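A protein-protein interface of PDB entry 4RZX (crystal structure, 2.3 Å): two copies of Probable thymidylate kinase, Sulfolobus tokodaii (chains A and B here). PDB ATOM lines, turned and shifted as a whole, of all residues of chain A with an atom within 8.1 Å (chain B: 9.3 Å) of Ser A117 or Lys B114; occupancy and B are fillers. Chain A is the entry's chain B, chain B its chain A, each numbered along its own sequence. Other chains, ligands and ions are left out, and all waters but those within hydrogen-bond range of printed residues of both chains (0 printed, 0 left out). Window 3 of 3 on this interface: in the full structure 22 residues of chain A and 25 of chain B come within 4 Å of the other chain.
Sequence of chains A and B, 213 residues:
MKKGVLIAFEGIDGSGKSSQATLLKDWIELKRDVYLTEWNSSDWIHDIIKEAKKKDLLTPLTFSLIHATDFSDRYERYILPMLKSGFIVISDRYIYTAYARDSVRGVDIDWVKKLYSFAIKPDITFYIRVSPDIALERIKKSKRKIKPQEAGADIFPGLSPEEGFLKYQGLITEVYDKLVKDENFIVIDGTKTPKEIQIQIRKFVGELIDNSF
Printed residues of chain B that touch a printed residue of chain A: Leu B61, Leu B65, Trp B111, Lys B114, Leu B115 and Ser B117. Hydrophobic or aromatic side chains of chain B within 4 Å of the printed part of chain A: Leu B61, Leu B65, Trp B111 and Leu B115. Printed residues of chain A that touch a printed residue of chain B: Trp A111, Lys A114, Leu A115, Ser A117 and Phe A118. Hydrophobic or aromatic side chains of chain A within 4 Å of the printed part of chain B: Trp A111, Leu A115 and Phe A118. Along chain A the printed residues that touch a printed residue of chain B span positions 111 to 118. Among the printed residues, no Asp or Glu carboxylate lies within 4 Å of a Lys or Arg side-chain nitrogen of the other chain.
The indole nitrogen (NE1) of Trp B111 is in hydrogen-bond range of the backbone carbonyl oxygen (O) of Lys A114, at 3.1 Å. The indole nitrogen of Trp A111 sits at hydrogen-bond distance from the backbone carbonyl oxygen of Lys B114 (3.2 Å). The indole nitrogen (NE1) of Trp B111 sits at hydrogen-bond distance from the backbone carbonyl oxygen (O) of Leu A115, at 3.1 Å. NE1 of Trp A111 sits at hydrogen-bond distance from OG of Ser B117 (3.2 Å).
Ser A117 touches just these residues of chain B: Trp B111 and Lys B114. Printed residues of chain A within 4 Å of Lys B114: Trp A111, Lys A114 and Ser A117. Lys A114 touches just these residues of chain B: Trp B111 and Lys B114. No residue of chain B comes within 4 Å of Ala A119. Printed residues of chain B within 4 Å of Leu A115: Leu B65, Trp B111 and Leu B115. Printed residues of chain A within 4 Å of Ser B117: Trp A111 (3.2 Å). Printed residues of chain A within 4 Å of Leu B61: Phe A118. Glu B183 touches none of the printed residues of chain A. Ala B119 touches none of the printed residues of chain A.
Among the printed residues, merely in contact across the chains: Trp A111 with Leu B115 (3.6 Å), Lys A114 with Lys B114 (3.8 Å), Leu A115 with Leu B65 (3.7 Å), Leu A115 with Leu B115 (3.9 Å), Ser A117 with Trp B111 (3.5 Å), Ser A117 with Lys B114 (3.6 Å), Phe A118 with Leu B61 (3.4 Å) and Phe A118 with Trp B111 (3.8 Å).
O of Lys B114 sits at hydrogen-bond distance from OG of Ser B117, 3.0 Å away. The side-chain carboxylate of Asp B108 lies within hydrogen-bond range of the backbone NH of Trp B111, at 3.3 Å.
Trp A111 touches Leu B115, and with the chains exchanged Leu A115 touches Trp B111. Lys B114 touches its own counterpart, Lys A114. Ser A117 touches Lys B114, but with the chains exchanged Lys A114 does not touch Ser B117 (7.7 Å). Phe A118 touches Trp B111, but with the chains exchanged Trp A111 does not touch Phe B118 (4.5 Å).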
ATOM      1  N   PHE A  71     -21.418   8.128 -28.149  1.00  0.00           N
ATOM      2  CA  PHE A  71     -22.377   8.990 -27.542  1.00  0.00           C
ATOM      3  C   PHE A  71     -22.048  10.458 -27.812  1.00  0.00           C
ATOM      4  O   PHE A  71     -22.956  11.247 -28.108  1.00  0.00           O
ATOM      5  CB  PHE A  71     -22.443   8.784 -26.040  1.00  0.00           C
ATOM      6  CG  PHE A  71     -23.409   9.700 -25.389  1.00  0.00           C
ATOM      7  CD1 PHE A  71     -24.741   9.395 -25.354  1.00  0.00           C
ATOM      8  CD2 PHE A  71     -23.001  10.900 -24.901  1.00  0.00           C
ATOM      9  CE1 PHE A  71     -25.657  10.285 -24.831  1.00  0.00           C
ATOM     10  CE2 PHE A  71     -23.896  11.776 -24.348  1.00  0.00           C
ATOM     11  CZ  PHE A  71     -25.223  11.479 -24.333  1.00  0.00           C
ATOM     12  N   TYR A  75     -24.423  13.171 -29.585  1.00  0.00           N
ATOM     13  CA  TYR A  75     -24.838  14.250 -28.699  1.00  0.00           C
ATOM     14  C   TYR A  75     -24.538  15.569 -29.388  1.00  0.00           C
ATOM     15  O   TYR A  75     -25.406  16.398 -29.544  1.00  0.00           O
ATOM     16  CB  TYR A  75     -24.144  14.174 -27.305  1.00  0.00           C
ATOM     17  CG  TYR A  75     -24.542  15.331 -26.339  1.00  0.00           C
ATOM     18  CD1 TYR A  75     -25.729  15.269 -25.588  1.00  0.00           C
ATOM     19  CD2 TYR A  75     -23.781  16.508 -26.260  1.00  0.00           C
ATOM     20  CE1 TYR A  75     -26.108  16.320 -24.759  1.00  0.00           C
ATOM     21  CE2 TYR A  75     -24.139  17.554 -25.400  1.00  0.00           C
ATOM     22  CZ  TYR A  75     -25.309  17.442 -24.674  1.00  0.00           C
ATOM     23  OH  TYR A  75     -25.675  18.441 -23.870  1.00  0.00           O
ATOM     24  N   ILE A  95     -27.262   8.873 -20.727  1.00  0.00           N
ATOM     25  CA  ILE A  95     -25.998   8.557 -20.016  1.00  0.00           C
ATOM     26  C   ILE A  95     -26.118   7.579 -18.864  1.00  0.00           C
ATOM     27  O   ILE A  95     -25.138   6.934 -18.458  1.00  0.00           O
ATOM     28  CB  ILE A  95     -25.313   9.814 -19.562  1.00  0.00           C
ATOM     29  CG1 ILE A  95     -26.092  10.509 -18.461  1.00  0.00           C
ATOM     30  CG2 ILE A  95     -25.148  10.748 -20.755  1.00  0.00           C
ATOM     31  CD1 ILE A  95     -25.388  11.797 -17.975  1.00  0.00           C
ATOM     32  N   TYR A  99     -23.855   4.669 -17.239  1.00  0.00           N
ATOM     33  CA  TYR A  99     -23.481   4.539 -15.836  1.00  0.00           C
ATOM     34  C   TYR A  99     -23.574   3.077 -15.390  1.00  0.00           C
ATOM     35  O   TYR A  99     -22.748   2.610 -14.628  1.00  0.00           O
ATOM     36  CB  TYR A  99     -24.380   5.372 -14.945  1.00  0.00           C
ATOM     37  CG  TYR A  99     -24.264   6.870 -15.049  1.00  0.00           C
ATOM     38  CD1 TYR A  99     -23.490   7.511 -16.037  1.00  0.00           C
ATOM     39  CD2 TYR A  99     -24.961   7.655 -14.159  1.00  0.00           C
ATOM     40  CE1 TYR A  99     -23.439   8.884 -16.101  1.00  0.00           C
ATOM     41  CE2 TYR A  99     -24.884   9.022 -14.192  1.00  0.00           C
ATOM     42  CZ  TYR A  99     -24.130   9.636 -15.159  1.00  0.00           C
ATOM     43  OH  TYR A  99     -24.137  11.006 -15.150  1.00  0.00           O
ATOM     44  N   ASP A 110     -18.344   7.245 -10.547  1.00  0.00           N
ATOM     45  CA  ASP A 110     -18.073   8.669 -10.486  1.00  0.00           C
ATOM     46  C   ASP A 110     -17.102   9.088 -11.603  1.00  0.00           C
ATOM     47  O   ASP A 110     -17.187  10.222 -12.097  1.00  0.00           O
ATOM     48  CB  ASP A 110     -17.596   9.087  -9.082  1.00  0.00           C
ATOM     49  CG  ASP A 110     -18.705   8.916  -8.029  1.00  0.00           C
ATOM     50  OD1 ASP A 110     -19.848   9.411  -8.231  1.00  0.00           O
ATOM     51  OD2 ASP A 110     -18.441   8.263  -6.994  1.00  0.00           O
ATOM     52  N   TRP A 111     -16.210   8.180 -12.010  1.00  0.00           N
ATOM     53  CA  TRP A 111     -15.366   8.438 -13.185  1.00  0.00           C
ATOM     54  C   TRP A 111     -16.266   8.504 -14.468  1.00  0.00           C
ATOM     55  O   TRP A 111     -16.191   9.445 -15.263  1.00  0.00           O
ATOM     56  CB  TRP A 111     -14.222   7.394 -13.342  1.00  0.00           C
ATOM     57  CG  TRP A 111     -13.350   7.713 -14.550  1.00  0.00           C
ATOM     58  CD1 TRP A 111     -12.328   8.605 -14.598  1.00  0.00           C
ATOM     59  CD2 TRP A 111     -13.483   7.189 -15.894  1.00  0.00           C
ATOM     60  NE1 TRP A 111     -11.802   8.649 -15.861  1.00  0.00           N
ATOM     61  CE2 TRP A 111     -12.492   7.803 -16.676  1.00  0.00           C
ATOM     62  CE3 TRP A 111     -14.330   6.253 -16.489  1.00  0.00           C
ATOM     63  CZ2 TRP A 111     -12.309   7.507 -18.024  1.00  0.00           C
ATOM     64  CZ3 TRP A 111     -14.180   5.979 -17.828  1.00  0.00           C
ATOM     65  CH2 TRP A 111     -13.166   6.594 -18.586  1.00  0.00           C
ATOM     66  N   VAL A 112     -17.130   7.528 -14.648  1.00  0.00           N
ATOM     67  CA  VAL A 112     -18.067   7.579 -15.773  1.00  0.00           C
ATOM     68  C   VAL A 112     -18.884   8.889 -15.752  1.00  0.00           C
ATOM     69  O   VAL A 112     -19.080   9.535 -16.788  1.00  0.00           O
ATOM     70  CB  VAL A 112     -19.012   6.373 -15.744  1.00  0.00           C
ATOM     71  CG1 VAL A 112     -19.911   6.366 -16.969  1.00  0.00           C
ATOM     72  CG2 VAL A 112     -18.212   5.086 -15.679  1.00  0.00           C
ATOM     73  N   LYS A 113     -19.372   9.299 -14.592  1.00  0.00           N
ATOM     74  CA  LYS A 113     -20.204  10.528 -14.532  1.00  0.00           C
ATOM     75  C   LYS A 113     -19.432  11.744 -15.076  1.00  0.00           C
ATOM     76  O   LYS A 113     -19.969  12.555 -15.853  1.00  0.00           O
ATOM     77  CB  LYS A 113     -20.700  10.807 -13.099  1.00  0.00           C
ATOM     78  CG  LYS A 113     -21.756   9.824 -12.584  1.00  0.00           C
ATOM     79  CD  LYS A 113     -22.052   9.867 -11.074  1.00  0.00           C
ATOM     80  CE  LYS A 113     -23.089   8.790 -10.736  1.00  0.00           C
ATOM     81  NZ  LYS A 113     -23.435   8.635  -9.285  1.00  0.00           N
ATOM     82  N   LYS A 114     -18.172  11.867 -14.654  1.00  0.00           N
ATOM     83  CA  LYS A 114     -17.296  12.972 -15.101  1.00  0.00           C
ATOM     84  C   LYS A 114     -17.041  12.920 -16.615  1.00  0.00           C
ATOM     85  O   LYS A 114     -17.164  13.939 -17.300  1.00  0.00           O
ATOM     86  CB  LYS A 114     -15.954  12.943 -14.338  1.00  0.00           C
ATOM     87  N   LEU A 115     -16.691  11.737 -17.111  1.00  0.00           N
ATOM     88  CA  LEU A 115     -16.632  11.422 -18.548  1.00  0.00           C
ATOM     89  C   LEU A 115     -17.831  11.999 -19.343  1.00  0.00           C
ATOM     90  O   LEU A 115     -17.637  12.682 -20.400  1.00  0.00           O
ATOM     91  CB  LEU A 115     -16.632   9.908 -18.747  1.00  0.00           C
ATOM     92  CG  LEU A 115     -16.782   9.432 -20.188  1.00  0.00           C
ATOM     93  CD1 LEU A 115     -15.639   9.909 -21.051  1.00  0.00           C
ATOM     94  CD2 LEU A 115     -16.833   7.917 -20.193  1.00  0.00           C
ATOM     95  N   TYR A 116     -19.040  11.763 -18.801  1.00  0.00           N
ATOM     96  CA  TYR A 116     -20.283  12.178 -19.480  1.00  0.00           C
ATOM     97  C   TYR A 116     -20.755  13.533 -19.041  1.00  0.00           C
ATOM     98  O   TYR A 116     -21.843  13.911 -19.424  1.00  0.00           O
ATOM     99  CB  TYR A 116     -21.406  11.161 -19.309  1.00  0.00           C
ATOM    100  CG  TYR A 116     -21.275   9.956 -20.221  1.00  0.00           C
ATOM    101  CD1 TYR A 116     -21.812   9.943 -21.508  1.00  0.00           C
ATOM    102  CD2 TYR A 116     -20.613   8.820 -19.789  1.00  0.00           C
ATOM    103  CE1 TYR A 116     -21.688   8.800 -22.350  1.00  0.00           C
ATOM    104  CE2 TYR A 116     -20.498   7.703 -20.601  1.00  0.00           C
ATOM    105  CZ  TYR A 116     -21.038   7.695 -21.866  1.00  0.00           C
ATOM    106  OH  TYR A 116     -20.840   6.565 -22.620  1.00  0.00           O
ATOM    107  N   SER A 117     -19.941  14.280 -18.276  1.00  0.00           N
ATOM    108  CA  SER A 117     -20.388  15.532 -17.710  1.00  0.00           C
ATOM    109  C   SER A 117     -20.536  16.668 -18.745  1.00  0.00           C
ATOM    110  O   SER A 117     -21.073  17.740 -18.438  1.00  0.00           O
ATOM    111  CB  SER A 117     -19.446  15.970 -16.565  1.00  0.00           C
ATOM    112  OG  SER A 117     -18.089  16.018 -16.958  1.00  0.00           O
ATOM    113  N   PHE A 118     -20.048  16.475 -19.958  1.00  0.00           N
ATOM    114  CA  PHE A 118     -20.383  17.417 -21.059  1.00  0.00           C
ATOM    115  C   PHE A 118     -21.863  17.361 -21.510  1.00  0.00           C
ATOM    116  O   PHE A 118     -22.338  18.267 -22.217  1.00  0.00           O
ATOM    117  CB  PHE A 118     -19.505  17.142 -22.273  1.00  0.00           C
ATOM    118  CG  PHE A 118     -19.656  15.745 -22.813  1.00  0.00           C
ATOM    119  CD1 PHE A 118     -20.722  15.415 -23.621  1.00  0.00           C
ATOM    120  CD2 PHE A 118     -18.756  14.767 -22.472  1.00  0.00           C
ATOM    121  CE1 PHE A 118     -20.883  14.130 -24.090  1.00  0.00           C
ATOM    122  CE2 PHE A 118     -18.881  13.488 -22.950  1.00  0.00           C
ATOM    123  CZ  PHE A 118     -19.950  13.151 -23.752  1.00  0.00           C
ATOM    124  N   ALA A 119     -22.595  16.315 -21.113  1.00  0.00           N
ATOM    125  CA  ALA A 119     -24.045  16.165 -21.484  1.00  0.00           C
ATOM    126  C   ALA A 119     -25.014  16.765 -20.473  1.00  0.00           C
ATOM    127  O   ALA A 119     -24.831  16.626 -19.292  1.00  0.00           O
ATOM    128  CB  ALA A 119     -24.398  14.709 -21.657  1.00  0.00           C
ATOM    129  N   ILE A 120     -26.073  17.384 -20.952  1.00  0.00           N
ATOM    130  CA  ILE A 120     -27.023  17.952 -20.055  1.00  0.00           C
ATOM    131  C   ILE A 120     -27.939  16.902 -19.446  1.00  0.00           C
ATOM    132  O   ILE A 120     -28.176  15.823 -20.017  1.00  0.00           O
ATOM    133  CB  ILE A 120     -27.761  19.118 -20.685  1.00  0.00           C
ATOM    134  CG1 ILE A 120     -28.636  18.672 -21.843  1.00  0.00           C
ATOM    135  CG2 ILE A 120     -26.739  20.158 -21.170  1.00  0.00           C
ATOM    136  CD1 ILE A 120     -29.508  19.817 -22.366  1.00  0.00           C
ATOM    137  N   LYS A 121     -28.412  17.235 -18.252  1.00  0.00           N
ATOM    138  CA  LYS A 121     -29.377  16.453 -17.551  1.00  0.00           C
ATOM    139  C   LYS A 121     -30.708  16.597 -18.285  1.00  0.00           C
ATOM    140  O   LYS A 121     -31.059  17.693 -18.746  1.00  0.00           O
ATOM    141  CB  LYS A 121     -29.495  16.955 -16.118  1.00  0.00           C
ATOM    142  CG  LYS A 121     -30.349  16.075 -15.207  1.00  0.00           C
ATOM    143  CD  LYS A 121     -30.406  16.616 -13.773  1.00  0.00           C
ATOM    144  CE  LYS A 121     -30.749  15.506 -12.789  1.00  0.00           C
ATOM    145  NZ  LYS A 121     -30.497  15.874 -11.352  1.00  0.00           N
ATOM    146  N   LEU B  61     -14.615  17.379 -29.068  1.00  0.00           N
ATOM    147  CA  LEU B  61     -14.832  16.509 -27.959  1.00  0.00           C
ATOM    148  C   LEU B  61     -14.647  15.063 -28.443  1.00  0.00           C
ATOM    149  O   LEU B  61     -13.941  14.243 -27.845  1.00  0.00           O
ATOM    150  CB  LEU B  61     -16.237  16.787 -27.399  1.00  0.00           C
ATOM    151  CG  LEU B  61     -16.768  15.869 -26.319  1.00  0.00           C
ATOM    152  CD1 LEU B  61     -15.799  15.871 -25.152  1.00  0.00           C
ATOM    153  CD2 LEU B  61     -18.124  16.399 -25.816  1.00  0.00           C
ATOM    154  N   LEU B  65     -12.029  12.073 -27.578  1.00  0.00           N
ATOM    155  CA  LEU B  65     -12.364  10.734 -27.068  1.00  0.00           C
ATOM    156  C   LEU B  65     -11.834   9.617 -27.950  1.00  0.00           C
ATOM    157  O   LEU B  65     -11.597   8.489 -27.492  1.00  0.00           O
ATOM    158  CB  LEU B  65     -13.860  10.592 -26.844  1.00  0.00           C
ATOM    159  CG  LEU B  65     -14.346  11.364 -25.624  1.00  0.00           C
ATOM    160  CD1 LEU B  65     -15.803  11.833 -25.755  1.00  0.00           C
ATOM    161  CD2 LEU B  65     -14.209  10.511 -24.397  1.00  0.00           C
ATOM    162  N   ALA B  68      -8.228   9.258 -26.667  1.00  0.00           N
ATOM    163  CA  ALA B  68      -8.204   8.655 -25.356  1.00  0.00           C
ATOM    164  C   ALA B  68      -8.607   7.185 -25.379  1.00  0.00           C
ATOM    165  O   ALA B  68      -7.998   6.363 -24.676  1.00  0.00           O
ATOM    166  CB  ALA B  68      -9.074   9.433 -24.418  1.00  0.00           C
ATOM    167  N   ILE B  95       0.246  11.904 -22.035  1.00  0.00           N
ATOM    168  CA  ILE B  95      -1.078  12.521 -21.875  1.00  0.00           C
ATOM    169  C   ILE B  95      -1.090  14.045 -21.997  1.00  0.00           C
ATOM    170  O   ILE B  95      -2.106  14.630 -22.432  1.00  0.00           O
ATOM    171  CB  ILE B  95      -1.758  12.099 -20.568  1.00  0.00           C
ATOM    172  CG1 ILE B  95      -1.023  12.632 -19.339  1.00  0.00           C
ATOM    173  CG2 ILE B  95      -1.912  10.574 -20.541  1.00  0.00           C
ATOM    174  CD1 ILE B  95      -1.592  12.075 -18.020  1.00  0.00           C
ATOM    175  N   TYR B  99      -3.729  16.881 -23.473  1.00  0.00           N
ATOM    176  CA  TYR B  99      -4.188  17.998 -22.731  1.00  0.00           C
ATOM    177  C   TYR B  99      -4.072  19.273 -23.602  1.00  0.00           C
ATOM    178  O   TYR B  99      -4.992  20.086 -23.676  1.00  0.00           O
ATOM    179  CB  TYR B  99      -3.295  18.259 -21.548  1.00  0.00           C
ATOM    180  CG  TYR B  99      -3.389  17.401 -20.320  1.00  0.00           C
ATOM    181  CD1 TYR B  99      -3.963  16.172 -20.326  1.00  0.00           C
ATOM    182  CD2 TYR B  99      -2.775  17.828 -19.147  1.00  0.00           C
ATOM    183  CE1 TYR B  99      -4.002  15.395 -19.182  1.00  0.00           C
ATOM    184  CE2 TYR B  99      -2.783  17.047 -18.013  1.00  0.00           C
ATOM    185  CZ  TYR B  99      -3.420  15.835 -18.032  1.00  0.00           C
ATOM    186  OH  TYR B  99      -3.449  15.056 -16.900  1.00  0.00           O
ATOM    187  N   ASP B 108     -12.519  21.515 -22.483  1.00  0.00           N
ATOM    188  CA  ASP B 108     -12.093  22.027 -21.180  1.00  0.00           C
ATOM    189  C   ASP B 108     -11.020  21.092 -20.617  1.00  0.00           C
ATOM    190  O   ASP B 108     -11.233  19.878 -20.482  1.00  0.00           O
ATOM    191  CB  ASP B 108     -13.318  22.154 -20.238  1.00  0.00           C
ATOM    192  CG  ASP B 108     -12.957  22.247 -18.718  1.00  0.00           C
ATOM    193  OD1 ASP B 108     -12.124  23.091 -18.310  1.00  0.00           O
ATOM    194  OD2 ASP B 108     -13.560  21.497 -17.914  1.00  0.00           O
ATOM    195  N   ILE B 109      -9.873  21.689 -20.285  1.00  0.00           N
ATOM    196  CA  ILE B 109      -8.665  20.958 -19.941  1.00  0.00           C
ATOM    197  C   ILE B 109      -8.913  20.122 -18.676  1.00  0.00           C
ATOM    198  O   ILE B 109      -8.465  18.949 -18.598  1.00  0.00           O
ATOM    199  CB  ILE B 109      -7.466  21.929 -19.838  1.00  0.00           C
ATOM    200  CG1 ILE B 109      -6.130  21.189 -19.905  1.00  0.00           C
ATOM    201  CG2 ILE B 109      -7.507  22.752 -18.541  1.00  0.00           C
ATOM    202  CD1 ILE B 109      -4.966  22.164 -20.034  1.00  0.00           C
ATOM    203  N   ASP B 110      -9.674  20.683 -17.720  1.00  0.00           N
ATOM    204  CA  ASP B 110     -10.009  19.963 -16.461  1.00  0.00           C
ATOM    205  C   ASP B 110     -10.790  18.673 -16.772  1.00  0.00           C
ATOM    206  O   ASP B 110     -10.478  17.596 -16.225  1.00  0.00           O
ATOM    207  CB  ASP B 110     -10.705  20.868 -15.399  1.00  0.00           C
ATOM    208  N   TRP B 111     -11.686  18.726 -17.747  1.00  0.00           N
ATOM    209  CA  TRP B 111     -12.336  17.500 -18.230  1.00  0.00           C
ATOM    210  C   TRP B 111     -11.338  16.519 -18.917  1.00  0.00           C
ATOM    211  O   TRP B 111     -11.362  15.301 -18.702  1.00  0.00           O
ATOM    212  CB  TRP B 111     -13.502  17.856 -19.139  1.00  0.00           C
ATOM    213  CG  TRP B 111     -14.251  16.679 -19.670  1.00  0.00           C
ATOM    214  CD1 TRP B 111     -15.293  16.064 -19.095  1.00  0.00           C
ATOM    215  CD2 TRP B 111     -13.987  15.980 -20.886  1.00  0.00           C
ATOM    216  NE1 TRP B 111     -15.712  15.007 -19.877  1.00  0.00           N
ATOM    217  CE2 TRP B 111     -14.928  14.958 -20.995  1.00  0.00           C
ATOM    218  CE3 TRP B 111     -13.096  16.182 -21.939  1.00  0.00           C
ATOM    219  CZ2 TRP B 111     -14.990  14.125 -22.083  1.00  0.00           C
ATOM    220  CZ3 TRP B 111     -13.159  15.352 -23.011  1.00  0.00           C
ATOM    221  CH2 TRP B 111     -14.088  14.325 -23.072  1.00  0.00           C
ATOM    222  N   VAL B 112     -10.436  17.019 -19.726  1.00  0.00           N
ATOM    223  CA  VAL B 112      -9.450  16.122 -20.313  1.00  0.00           C
ATOM    224  C   VAL B 112      -8.577  15.452 -19.232  1.00  0.00           C
ATOM    225  O   VAL B 112      -8.266  14.295 -19.355  1.00  0.00           O
ATOM    226  CB  VAL B 112      -8.570  16.895 -21.325  1.00  0.00           C
ATOM    227  CG1 VAL B 112      -7.478  16.004 -21.908  1.00  0.00           C
ATOM    228  CG2 VAL B 112      -9.440  17.451 -22.427  1.00  0.00           C
ATOM    229  N   LYS B 113      -8.205  16.182 -18.177  1.00  0.00           N
ATOM    230  CA  LYS B 113      -7.419  15.641 -17.102  1.00  0.00           C
ATOM    231  C   LYS B 113      -8.144  14.508 -16.422  1.00  0.00           C
ATOM    232  O   LYS B 113      -7.567  13.439 -16.195  1.00  0.00           O
ATOM    233  CB  LYS B 113      -7.033  16.728 -16.059  1.00  0.00           C
ATOM    234  CG  LYS B 113      -5.820  17.607 -16.402  1.00  0.00           C
ATOM    235  CD  LYS B 113      -5.738  18.892 -15.554  1.00  0.00           C
ATOM    236  N   LYS B 114      -9.416  14.737 -16.120  1.00  0.00           N
ATOM    237  CA  LYS B 114     -10.307  13.691 -15.601  1.00  0.00           C
ATOM    238  C   LYS B 114     -10.323  12.548 -16.582  1.00  0.00           C
ATOM    239  O   LYS B 114     -10.144  11.385 -16.181  1.00  0.00           O
ATOM    240  CB  LYS B 114     -11.746  14.209 -15.376  1.00  0.00           C
ATOM    241  CG  LYS B 114     -11.926  15.243 -14.244  1.00  0.00           C
ATOM    242  CD  LYS B 114     -13.395  15.696 -14.079  1.00  0.00           C
ATOM    243  CE  LYS B 114     -13.731  17.016 -14.769  1.00  0.00           C
ATOM    244  NZ  LYS B 114     -15.183  17.116 -15.112  1.00  0.00           N
ATOM    245  N   LEU B 115     -10.476  12.867 -17.869  1.00  0.00           N
ATOM    246  CA  LEU B 115     -10.589  11.807 -18.909  1.00  0.00           C
ATOM    247  C   LEU B 115      -9.389  10.853 -18.882  1.00  0.00           C
ATOM    248  O   LEU B 115      -9.529   9.648 -18.999  1.00  0.00           O
ATOM    249  CB  LEU B 115     -10.781  12.438 -20.285  1.00  0.00           C
ATOM    250  CG  LEU B 115     -10.733  11.632 -21.584  1.00  0.00           C
ATOM    251  CD1 LEU B 115     -11.911  10.688 -21.661  1.00  0.00           C
ATOM    252  CD2 LEU B 115     -10.778  12.553 -22.816  1.00  0.00           C
ATOM    253  N   TYR B 116      -8.197  11.402 -18.722  1.00  0.00           N
ATOM    254  CA  TYR B 116      -7.004  10.605 -18.690  1.00  0.00           C
ATOM    255  C   TYR B 116      -6.558  10.151 -17.293  1.00  0.00           C
ATOM    256  O   TYR B 116      -5.450   9.553 -17.158  1.00  0.00           O
ATOM    257  CB  TYR B 116      -5.862  11.388 -19.357  1.00  0.00           C
ATOM    258  CG  TYR B 116      -5.943  11.330 -20.829  1.00  0.00           C
ATOM    259  CD1 TYR B 116      -5.458  10.236 -21.496  1.00  0.00           C
ATOM    260  CD2 TYR B 116      -6.565  12.357 -21.580  1.00  0.00           C
ATOM    261  CE1 TYR B 116      -5.553  10.148 -22.853  1.00  0.00           C
ATOM    262  CE2 TYR B 116      -6.640  12.296 -22.982  1.00  0.00           C
ATOM    263  CZ  TYR B 116      -6.121  11.199 -23.609  1.00  0.00           C
ATOM    264  OH  TYR B 116      -6.199  11.010 -24.980  1.00  0.00           O
ATOM    265  N   SER B 117      -7.390  10.409 -16.278  1.00  0.00           N
ATOM    266  CA  SER B 117      -7.045  10.162 -14.857  1.00  0.00           C
ATOM    267  C   SER B 117      -6.626   8.730 -14.602  1.00  0.00           C
ATOM    268  O   SER B 117      -6.003   8.445 -13.582  1.00  0.00           O
ATOM    269  CB  SER B 117      -8.250  10.411 -13.969  1.00  0.00           C
ATOM    270  OG  SER B 117      -9.167   9.345 -14.181  1.00  0.00           O
ATOM    271  N   PHE B 118      -7.002   7.838 -15.522  1.00  0.00           N
ATOM    272  CA  PHE B 118      -6.674   6.440 -15.433  1.00  0.00           C
ATOM    273  C   PHE B 118      -5.229   6.114 -15.699  1.00  0.00           C
ATOM    274  O   PHE B 118      -4.819   4.992 -15.457  1.00  0.00           O
ATOM    275  CB  PHE B 118      -7.543   5.612 -16.393  1.00  0.00           C
ATOM    276  CG  PHE B 118      -7.223   5.815 -17.841  1.00  0.00           C
ATOM    277  CD1 PHE B 118      -6.191   5.150 -18.431  1.00  0.00           C
ATOM    278  CD2 PHE B 118      -7.970   6.691 -18.619  1.00  0.00           C
ATOM    279  CE1 PHE B 118      -5.877   5.358 -19.752  1.00  0.00           C
ATOM    280  CE2 PHE B 118      -7.668   6.901 -19.958  1.00  0.00           C
ATOM    281  CZ  PHE B 118      -6.636   6.217 -20.531  1.00  0.00           C
ATOM    282  N   ALA B 119      -4.452   7.039 -16.243  1.00  0.00           N
ATOM    283  CA  ALA B 119      -3.057   6.749 -16.548  1.00  0.00           C
ATOM    284  C   ALA B 119      -2.214   7.281 -15.415  1.00  0.00           C
ATOM    285  O   ALA B 119      -2.558   8.265 -14.794  1.00  0.00           O
ATOM    286  CB  ALA B 119      -2.619   7.375 -17.853  1.00  0.00           C
ATOM    287  N   GLU B 183       2.542  19.706 -12.842  1.00  0.00           N
ATOM    288  CA  GLU B 183       2.887  18.376 -13.315  1.00  0.00           C
ATOM    289  C   GLU B 183       4.364  18.030 -12.997  1.00  0.00           C
ATOM    290  O   GLU B 183       4.873  16.983 -13.388  1.00  0.00           O
ATOM    291  CB  GLU B 183       2.569  18.282 -14.791  1.00  0.00           C
ATOM    292  CG  GLU B 183       1.107  18.586 -15.150  1.00  0.00           C
ATOM    293  CD  GLU B 183       0.122  17.624 -14.460  1.00  0.00           C
ATOM    294  OE1 GLU B 183       0.560  16.517 -14.043  1.00  0.00           O
ATOM    295  OE2 GLU B 183      -1.087  17.967 -14.310  1.00  0.00           O
